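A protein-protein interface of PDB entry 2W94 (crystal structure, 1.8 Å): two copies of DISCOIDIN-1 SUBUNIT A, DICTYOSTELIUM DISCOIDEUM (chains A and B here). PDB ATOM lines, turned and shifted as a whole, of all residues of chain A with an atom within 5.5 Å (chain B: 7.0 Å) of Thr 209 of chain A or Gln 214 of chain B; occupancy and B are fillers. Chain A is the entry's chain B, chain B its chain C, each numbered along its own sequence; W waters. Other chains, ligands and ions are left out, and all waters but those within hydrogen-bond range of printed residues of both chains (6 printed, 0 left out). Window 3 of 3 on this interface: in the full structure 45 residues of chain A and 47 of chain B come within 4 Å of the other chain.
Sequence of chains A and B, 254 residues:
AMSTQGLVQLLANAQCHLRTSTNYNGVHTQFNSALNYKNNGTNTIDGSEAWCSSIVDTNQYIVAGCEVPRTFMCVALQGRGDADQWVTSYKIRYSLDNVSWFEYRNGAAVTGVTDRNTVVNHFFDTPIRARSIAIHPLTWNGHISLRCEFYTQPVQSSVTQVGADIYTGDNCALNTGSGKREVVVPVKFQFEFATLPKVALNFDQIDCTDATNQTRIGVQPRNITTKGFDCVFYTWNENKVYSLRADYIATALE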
ATOM      1  N   ASN A 175     -20.907  22.314   6.215  1.00  0.00           N
ATOM      2  CA  ASN A 175     -19.552  22.233   5.714  1.00  0.00           C
ATOM      3  C   ASN A 175     -19.251  23.355   4.723  1.00  0.00           C
ATOM      4  O   ASN A 175     -18.186  23.364   4.098  1.00  0.00           O
ATOM      5  CB  ASN A 175     -19.301  20.875   5.059  1.00  0.00           C
ATOM      6  CG  ASN A 175     -17.823  20.498   5.021  1.00  0.00           C
ATOM      7  OD1 ASN A 175     -17.052  20.927   5.861  1.00  0.00           O
ATOM      8  ND2 ASN A 175     -17.433  19.691   4.032  1.00  0.00           N
ATOM      9  N   ASP A 207     -16.814  15.521  13.272  1.00  0.00           N
ATOM     10  CA  ASP A 207     -15.921  15.624  12.090  1.00  0.00           C
ATOM     11  C   ASP A 207     -16.003  17.086  11.669  1.00  0.00           C
ATOM     12  O   ASP A 207     -16.909  17.479  10.924  1.00  0.00           O
ATOM     13  CB  ASP A 207     -16.434  14.742  10.953  1.00  0.00           C
ATOM     14  CG  ASP A 207     -15.364  14.483   9.852  1.00  0.00           C
ATOM     15  OD1 ASP A 207     -14.452  15.351   9.659  1.00  0.00           O
ATOM     16  OD2 ASP A 207     -15.472  13.435   9.170  1.00  0.00           O
ATOM     17  N   CYS A 208     -15.108  17.916  12.192  1.00  0.00           N
ATOM     18  CA  CYS A 208     -15.237  19.344  11.969  1.00  0.00           C
ATOM     19  C   CYS A 208     -13.875  20.031  11.779  1.00  0.00           C
ATOM     20  O   CYS A 208     -12.855  19.532  12.250  1.00  0.00           O
ATOM     21  CB  CYS A 208     -15.995  19.978  13.125  1.00  0.00           C
ATOM     22  SG  CYS A 208     -15.206  19.948  14.692  1.00  0.00           S
ATOM     23  N   THR A 209     -13.893  21.206  11.149  1.00  0.00           N
ATOM     24  CA  THR A 209     -12.658  21.995  10.944  1.00  0.00           C
ATOM     25  C   THR A 209     -12.669  23.199  11.829  1.00  0.00           C
ATOM     26  O   THR A 209     -13.700  23.856  11.957  1.00  0.00           O
ATOM     27  CB  THR A 209     -12.564  22.589   9.536  1.00  0.00           C
ATOM     28  OG1 THR A 209     -12.934  21.612   8.542  1.00  0.00           O
ATOM     29  CG2 THR A 209     -11.146  23.118   9.288  1.00  0.00           C
ATOM     30  N   ASP A 210     -11.534  23.520  12.439  1.00  0.00           N
ATOM     31  CA  ASP A 210     -11.453  24.752  13.216  1.00  0.00           C
ATOM     32  C   ASP A 210     -11.372  25.989  12.312  1.00  0.00           C
ATOM     33  O   ASP A 210     -11.164  25.864  11.096  1.00  0.00           O
ATOM     34  CB  ASP A 210     -10.287  24.706  14.233  1.00  0.00           C
ATOM     35  CG  ASP A 210      -8.922  24.650  13.577  1.00  0.00           C
ATOM     36  OD1 ASP A 210      -8.820  24.949  12.375  1.00  0.00           O
ATOM     37  OD2 ASP A 210      -7.943  24.357  14.284  1.00  0.00           O
ATOM     38  N   ALA A 211     -11.618  27.149  12.910  1.00  0.00           N
ATOM     39  CA  ALA A 211     -11.501  28.456  12.274  1.00  0.00           C
ATOM     40  C   ALA A 211     -10.663  29.333  13.231  1.00  0.00           C
ATOM     41  O   ALA A 211     -11.065  29.650  14.360  1.00  0.00           O
ATOM     42  CB  ALA A 211     -12.868  29.077  12.052  1.00  0.00           C
ATOM     43  N   GLN A 214     -10.276  27.858  16.484  1.00  0.00           N
ATOM     44  CA  GLN A 214     -11.493  27.711  17.305  1.00  0.00           C
ATOM     45  C   GLN A 214     -12.382  26.569  16.794  1.00  0.00           C
ATOM     46  O   GLN A 214     -12.631  26.447  15.603  1.00  0.00           O
ATOM     47  CB  GLN A 214     -12.307  28.980  17.276  1.00  0.00           C
ATOM     48  CG  GLN A 214     -13.245  29.136  18.477  1.00  0.00           C
ATOM     49  CD  GLN A 214     -12.503  29.499  19.759  1.00  0.00           C
ATOM     50  OE1 GLN A 214     -11.288  29.745  19.733  1.00  0.00           O
ATOM     51  NE2 GLN A 214     -13.213  29.510  20.888  1.00  0.00           N
ATOM     52  N   ASN A 239     -16.693  28.562  10.760  1.00  0.00           N
ATOM     53  CA  ASN A 239     -16.377  27.158  10.884  1.00  0.00           C
ATOM     54  C   ASN A 239     -17.063  26.289   9.868  1.00  0.00           C
ATOM     55  O   ASN A 239     -18.193  26.525   9.516  1.00  0.00           O
ATOM     56  CB  ASN A 239     -16.740  26.641  12.274  1.00  0.00           C
ATOM     57  CG  ASN A 239     -15.812  27.140  13.318  1.00  0.00           C
ATOM     58  OD1 ASN A 239     -15.884  28.307  13.695  1.00  0.00           O
ATOM     59  ND2 ASN A 239     -14.931  26.261  13.816  1.00  0.00           N
ATOM     60  N   LYS A 240     -16.372  25.255   9.428  1.00  0.00           N
ATOM     61  CA  LYS A 240     -16.910  24.291   8.507  1.00  0.00           C
ATOM     62  C   LYS A 240     -16.982  22.964   9.237  1.00  0.00           C
ATOM     63  O   LYS A 240     -15.961  22.456   9.740  1.00  0.00           O
ATOM     64  CB  LYS A 240     -16.008  24.162   7.263  1.00  0.00           C
ATOM     65  CG  LYS A 240     -15.653  25.509   6.631  1.00  0.00           C
ATOM     66  CD  LYS A 240     -16.871  26.149   5.938  1.00  0.00           C
ATOM     67  CE  LYS A 240     -16.475  27.364   5.056  1.00  0.00           C
ATOM     68  NZ  LYS A 240     -16.789  28.637   5.713  1.00  0.00           N
ATOM     69  N   VAL A 241     -18.185  22.399   9.268  1.00  0.00           N
ATOM     70  CA  VAL A 241     -18.457  21.128   9.913  1.00  0.00           C
ATOM     71  C   VAL A 241     -18.916  20.080   8.903  1.00  0.00           C
ATOM     72  O   VAL A 241     -19.965  20.190   8.217  1.00  0.00           O
ATOM     73  CB  VAL A 241     -19.520  21.300  11.056  1.00  0.00           C
ATOM     74  CG1 VAL A 241     -19.860  19.983  11.656  1.00  0.00           C
ATOM     75  CG2 VAL A 241     -19.067  22.296  12.146  1.00  0.00           C
ATOM     76  N   TYR A 242     -18.117  19.039   8.774  1.00  0.00           N
ATOM     77  CA  TYR A 242     -18.402  17.983   7.790  1.00  0.00           C
ATOM     78  C   TYR A 242     -19.621  17.141   8.179  1.00  0.00           C
ATOM     79  O   TYR A 242     -20.529  16.841   7.347  1.00  0.00           O
ATOM     80  CB  TYR A 242     -17.173  17.080   7.648  1.00  0.00           C
ATOM     81  CG  TYR A 242     -17.311  15.998   6.585  1.00  0.00           C
ATOM     82  CD1 TYR A 242     -17.103  16.270   5.230  1.00  0.00           C
ATOM     83  CD2 TYR A 242     -17.660  14.697   6.953  1.00  0.00           C
ATOM     84  CE1 TYR A 242     -17.227  15.256   4.263  1.00  0.00           C
ATOM     85  CE2 TYR A 242     -17.784  13.695   6.023  1.00  0.00           C
ATOM     86  CZ  TYR A 242     -17.566  13.969   4.684  1.00  0.00           C
ATOM     87  OH  TYR A 242     -17.709  12.934   3.789  1.00  0.00           O
ATOM     88  N   THR B 209      -5.655  15.745  19.060  1.00  0.00           N
ATOM     89  CA  THR B 209      -4.926  16.620  18.143  1.00  0.00           C
ATOM     90  C   THR B 209      -5.619  16.702  16.778  1.00  0.00           C
ATOM     91  O   THR B 209      -6.022  15.708  16.252  1.00  0.00           O
ATOM     92  CB  THR B 209      -3.498  16.092  17.832  1.00  0.00           C
ATOM     93  OG1 THR B 209      -2.851  15.631  19.021  1.00  0.00           O
ATOM     94  CG2 THR B 209      -2.669  17.219  17.231  1.00  0.00           C
ATOM     95  N   ASP B 210      -5.746  17.900  16.222  1.00  0.00           N
ATOM     96  CA  ASP B 210      -6.307  18.064  14.892  1.00  0.00           C
ATOM     97  C   ASP B 210      -5.315  17.545  13.846  1.00  0.00           C
ATOM     98  O   ASP B 210      -4.129  17.329  14.138  1.00  0.00           O
ATOM     99  CB  ASP B 210      -6.728  19.527  14.640  1.00  0.00           C
ATOM    100  CG  ASP B 210      -5.545  20.521  14.718  1.00  0.00           C
ATOM    101  OD1 ASP B 210      -4.406  20.113  14.386  1.00  0.00           O
ATOM    102  OD2 ASP B 210      -5.764  21.676  15.146  1.00  0.00           O
ATOM    103  N   ALA B 211      -5.834  17.233  12.669  1.00  0.00           N
ATOM    104  CA  ALA B 211      -5.018  16.863  11.520  1.00  0.00           C
ATOM    105  C   ALA B 211      -5.466  17.752  10.350  1.00  0.00           C
ATOM    106  O   ALA B 211      -6.606  17.695   9.897  1.00  0.00           O
ATOM    107  CB  ALA B 211      -5.172  15.396  11.198  1.00  0.00           C
ATOM    108  N   THR B 212      -4.551  18.606   9.889  1.00  0.00           N
ATOM    109  CA  THR B 212      -4.884  19.715   8.985  1.00  0.00           C
ATOM    110  C   THR B 212      -6.155  20.401   9.421  1.00  0.00           C
ATOM    111  O   THR B 212      -7.085  20.557   8.640  1.00  0.00           O
ATOM    112  CB  THR B 212      -5.022  19.306   7.517  1.00  0.00           C
ATOM    113  OG1 THR B 212      -3.963  18.422   7.148  1.00  0.00           O
ATOM    114  CG2 THR B 212      -4.977  20.576   6.605  1.00  0.00           C
ATOM    115  N   ASN B 213      -6.173  20.805  10.685  1.00  0.00           N
ATOM    116  CA  ASN B 213      -7.254  21.591  11.241  1.00  0.00           C
ATOM    117  C   ASN B 213      -8.566  20.833  11.468  1.00  0.00           C
ATOM    118  O   ASN B 213      -9.548  21.442  11.905  1.00  0.00           O
ATOM    119  CB  ASN B 213      -7.550  22.802  10.357  1.00  0.00           C
ATOM    120  CG  ASN B 213      -6.385  23.805  10.332  1.00  0.00           C
ATOM    121  OD1 ASN B 213      -5.561  23.830  11.232  1.00  0.00           O
ATOM    122  ND2 ASN B 213      -6.342  24.619   9.322  1.00  0.00           N
ATOM    123  N   GLN B 214      -8.572  19.536  11.156  1.00  0.00           N
ATOM    124  CA  GLN B 214      -9.780  18.703  11.292  1.00  0.00           C
ATOM    125  C   GLN B 214      -9.768  17.904  12.586  1.00  0.00           C
ATOM    126  O   GLN B 214      -8.762  17.239  12.929  1.00  0.00           O
ATOM    127  CB  GLN B 214      -9.882  17.723  10.128  1.00  0.00           C
ATOM    128  CG  GLN B 214     -11.295  17.179   9.895  1.00  0.00           C
ATOM    129  CD  GLN B 214     -12.205  18.206   9.296  1.00  0.00           C
ATOM    130  OE1 GLN B 214     -11.769  19.320   8.927  1.00  0.00           O
ATOM    131  NE2 GLN B 214     -13.483  17.863   9.179  1.00  0.00           N
ATOM    132  N   THR B 215     -10.888  17.972  13.312  1.00  0.00           N
ATOM    133  CA  THR B 215     -11.126  17.097  14.464  1.00  0.00           C
ATOM    134  C   THR B 215     -11.962  15.878  14.007  1.00  0.00           C
ATOM    135  O   THR B 215     -12.943  16.014  13.257  1.00  0.00           O
ATOM    136  CB  THR B 215     -11.885  17.841  15.577  1.00  0.00           C
ATOM    137  OG1 THR B 215     -11.073  18.885  16.110  1.00  0.00           O
ATOM    138  CG2 THR B 215     -12.282  16.881  16.721  1.00  0.00           C
ATOM    139  N   ARG B 216     -11.558  14.691  14.441  1.00  0.00           N
ATOM    140  CA  ARG B 216     -12.208  13.454  14.035  1.00  0.00           C
ATOM    141  C   ARG B 216     -12.269  12.510  15.233  1.00  0.00           C
ATOM    142  O   ARG B 216     -11.247  11.881  15.603  1.00  0.00           O
ATOM    143  CB  ARG B 216     -11.460  12.792  12.894  1.00  0.00           C
ATOM    144  CG  ARG B 216     -11.570  13.483  11.551  1.00  0.00           C
ATOM    145  CD  ARG B 216     -10.870  12.696  10.445  1.00  0.00           C
ATOM    146  NE  ARG B 216     -10.899  13.437   9.177  1.00  0.00           N
ATOM    147  CZ  ARG B 216      -9.906  14.167   8.696  1.00  0.00           C
ATOM    148  NH1 ARG B 216      -8.763  14.293   9.371  1.00  0.00           N
ATOM    149  NH2 ARG B 216     -10.066  14.788   7.542  1.00  0.00           N
ATOM    150  N   ASN B 237      -8.522   8.720   9.557  1.00  0.00           N
ATOM    151  CA  ASN B 237      -7.554   9.565   8.865  1.00  0.00           C
ATOM    152  C   ASN B 237      -6.241   9.609   9.680  1.00  0.00           C
ATOM    153  O   ASN B 237      -5.823   8.593  10.245  1.00  0.00           O
ATOM    154  CB  ASN B 237      -8.160  10.950   8.657  1.00  0.00           C
ATOM    155  CG  ASN B 237      -7.498  11.729   7.518  1.00  0.00           C
ATOM    156  OD1 ASN B 237      -6.405  12.266   7.679  1.00  0.00           O
ATOM    157  ND2 ASN B 237      -8.184  11.827   6.393  1.00  0.00           N
ATOM    158  N   ASN B 239      -5.588  11.583  12.343  1.00  0.00           N
ATOM    159  CA  ASN B 239      -5.740  12.164  13.669  1.00  0.00           C
ATOM    160  C   ASN B 239      -5.139  11.337  14.757  1.00  0.00           C
ATOM    161  O   ASN B 239      -5.192  10.105  14.730  1.00  0.00           O
ATOM    162  CB  ASN B 239      -7.208  12.419  13.980  1.00  0.00           C
ATOM    163  CG  ASN B 239      -7.805  13.448  13.063  1.00  0.00           C
ATOM    164  OD1 ASN B 239      -7.967  13.193  11.868  1.00  0.00           O
ATOM    165  ND2 ASN B 239      -8.100  14.608  13.590  1.00  0.00           N
HETATM  166  O   HOH W   1      -8.625  22.163  16.458  1.00  0.00           O
HETATM  167  O   HOH W   2     -10.414  21.014  14.553  1.00  0.00           O
HETATM  168  O   HOH W   3     -13.425  14.982   7.240  1.00  0.00           O
HETATM  169  O   HOH W   4     -13.680  12.455   7.664  1.00  0.00           O
HETATM  170  O   HOH W   5      -9.015  26.223   9.684  1.00  0.00           O
HETATM  171  O   HOH W   6     -15.300  19.983   7.821  1.00  0.00           O
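The backbone NH of Thr 209 of chain A sits at hydrogen-bond distance from the backbone carbonyl oxygen of Lys 240 of chain A, at 2.8 Å.
The side-chain amide nitrogen of Asn 239 of chain B sits at hydrogen-bond distance from the backbone carbonyl oxygen of Gln 214 of chain B (2.8 Å).
OD1 of Asn 239 of chain B sits at hydrogen-bond distance from NH1 of Arg 216 of chain B (2.8 Å).
The backbone carbonyl oxygen (O) of Thr 209 of chain A sits at hydrogen-bond distance from the side-chain amide nitrogen (ND2) of Asn 239 of chain A (3.3 Å).
O of Asp 207 of chain A lies within hydrogen-bond range of N of Tyr 242 of chain A, 2.9 Å away.
Of chain B, only Asn 213 (3.3 Å) and Gln 214 (2.6 Å) come within 4 Å of Thr 209 of chain A.
Gln 214 of chain B touches just these residues of chain A: Asp 207 (2.7 Å), Cys 208 (3.3 Å) and Thr 209 (2.6 Å).
Of the printed residues of chain B, Asp 210 of chain A touches Asp 210 and Asn 213.
Of the printed residues of chain A, Asn 213 of chain B touches Cys 208, Thr 209 and Asp 210.
Of the printed residues of chain B, Cys 208 of chain A touches Asn 213 (3.8 Å), Gln 214 (3.3 Å) and Thr 215 (2.7 Å).
Of the printed residues of chain A, Thr 215 of chain B touches Asp 207 and Cys 208.
Of the printed residues of chain A, Arg 216 of chain B touches Asp 207 (3.9 Å).
Asn 237 of chain B touches none of the printed residues of chain A.
Asn 239 of chain B touches none of the printed residues of chain A.
The nearest residue of chain B that does not touch Thr 209 of chain A is Thr 212 of chain B (4.8 Å).
The nearest printed residue of chain B that does not touch Cys 208 of chain A is Arg 216 of chain B (5.3 Å).
Printed residues of chain A that touch a printed residue of chain B: Asp 207, Cys 208, Thr 209 and Asp 210.
Along chain A the printed residues that touch a printed residue of chain B span positions 207 to 210.
Among the printed residues, no Asp or Glu carboxylate lies within 4 Å of a Lys or Arg side-chain nitrogen of the other chain.
Thr 209 of chain A touches Gln 214 of chain B, but with the chains exchanged Gln 214 of chain A does not touch Thr 209 of chain B (12.0 Å).
Asp 210 of chain A touches its own counterpart, Asp 210 of chain B.
Positions printed for both chains: 209, 210, 211, 214 and 239.
Of the 10 pairs that touch across the chains among the printed residues, 1 has its exchanged pair printed and touching as well.
Water W4 lies within hydrogen-bond range of OD2 of Asp 207 of chain A and NE of Arg 216 of chain B.
Water W5 bridges O of Asp 210 of chain A (2.6 Å) and ND2 of Asn 213 of chain B (3.1 Å).
Water W3 lies within hydrogen-bond range of OD1 of Asp 207 of chain A (2.7 Å), NH2 of Arg 216 of chain B (3.4 Å) and NE2 of Gln 214 of chain B (3.5 Å).
Water W2 lies within hydrogen-bond range of OG1 of Thr 215 of chain B (2.7 Å), O of Asn 213 of chain B (2.8 Å) and N of Asp 210 of chain A (3.5 Å).
Water W6 lies within hydrogen-bond range of OD1 of Asn 175 of chain A (2.8 Å), OG1 of Thr 209 of chain A (3.0 Å), NE2 of Gln 214 of chain B (3.1 Å), N of Tyr 242 of chain A (3.1 Å) and O of Lys 240 of chain A (3.2 Å).
Water W1 lies within hydrogen-bond range of the side-chain carboxylate of Asp 210 of chain A (3.2 Å) and the side-chain carboxylate of Asp 210 of chain B (3.2 Å).
Among the printed residues, pairs that only touch across the chains: Asp 207 of chain A with Thr 215 of chain B, Asp 207 of chain A with Arg 216 of chain B, Cys 208 of chain A with Asn 213 of chain B, Thr 209 of chain A with Asn 213 of chain B and Asp 210 of chain A with Asp 210 of chain B.
The side-chain carboxylate of Asp 207 of chain A sits at hydrogen-bond distance from the side-chain amide nitrogen of Gln 214 of chain B (2.7 Å).
The backbone carbonyl oxygen (O) of Cys 208 of chain A sits at hydrogen-bond distance from the backbone NH (N) of Thr 215 of chain B (2.7 Å).
OG1 of Thr 209 of chain A sits at hydrogen-bond distance from OE1 of Gln 214 of chain B, at 2.6 Å.
The backbone NH (N) of Cys 208 of chain A lies close to the side-chain amide nitrogen (NE2) of Gln 214 of chain B (3.4 Å).
N of Asp 210 of chain A lies within hydrogen-bond range of O of Asn 213 of chain B (2.9 Å).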
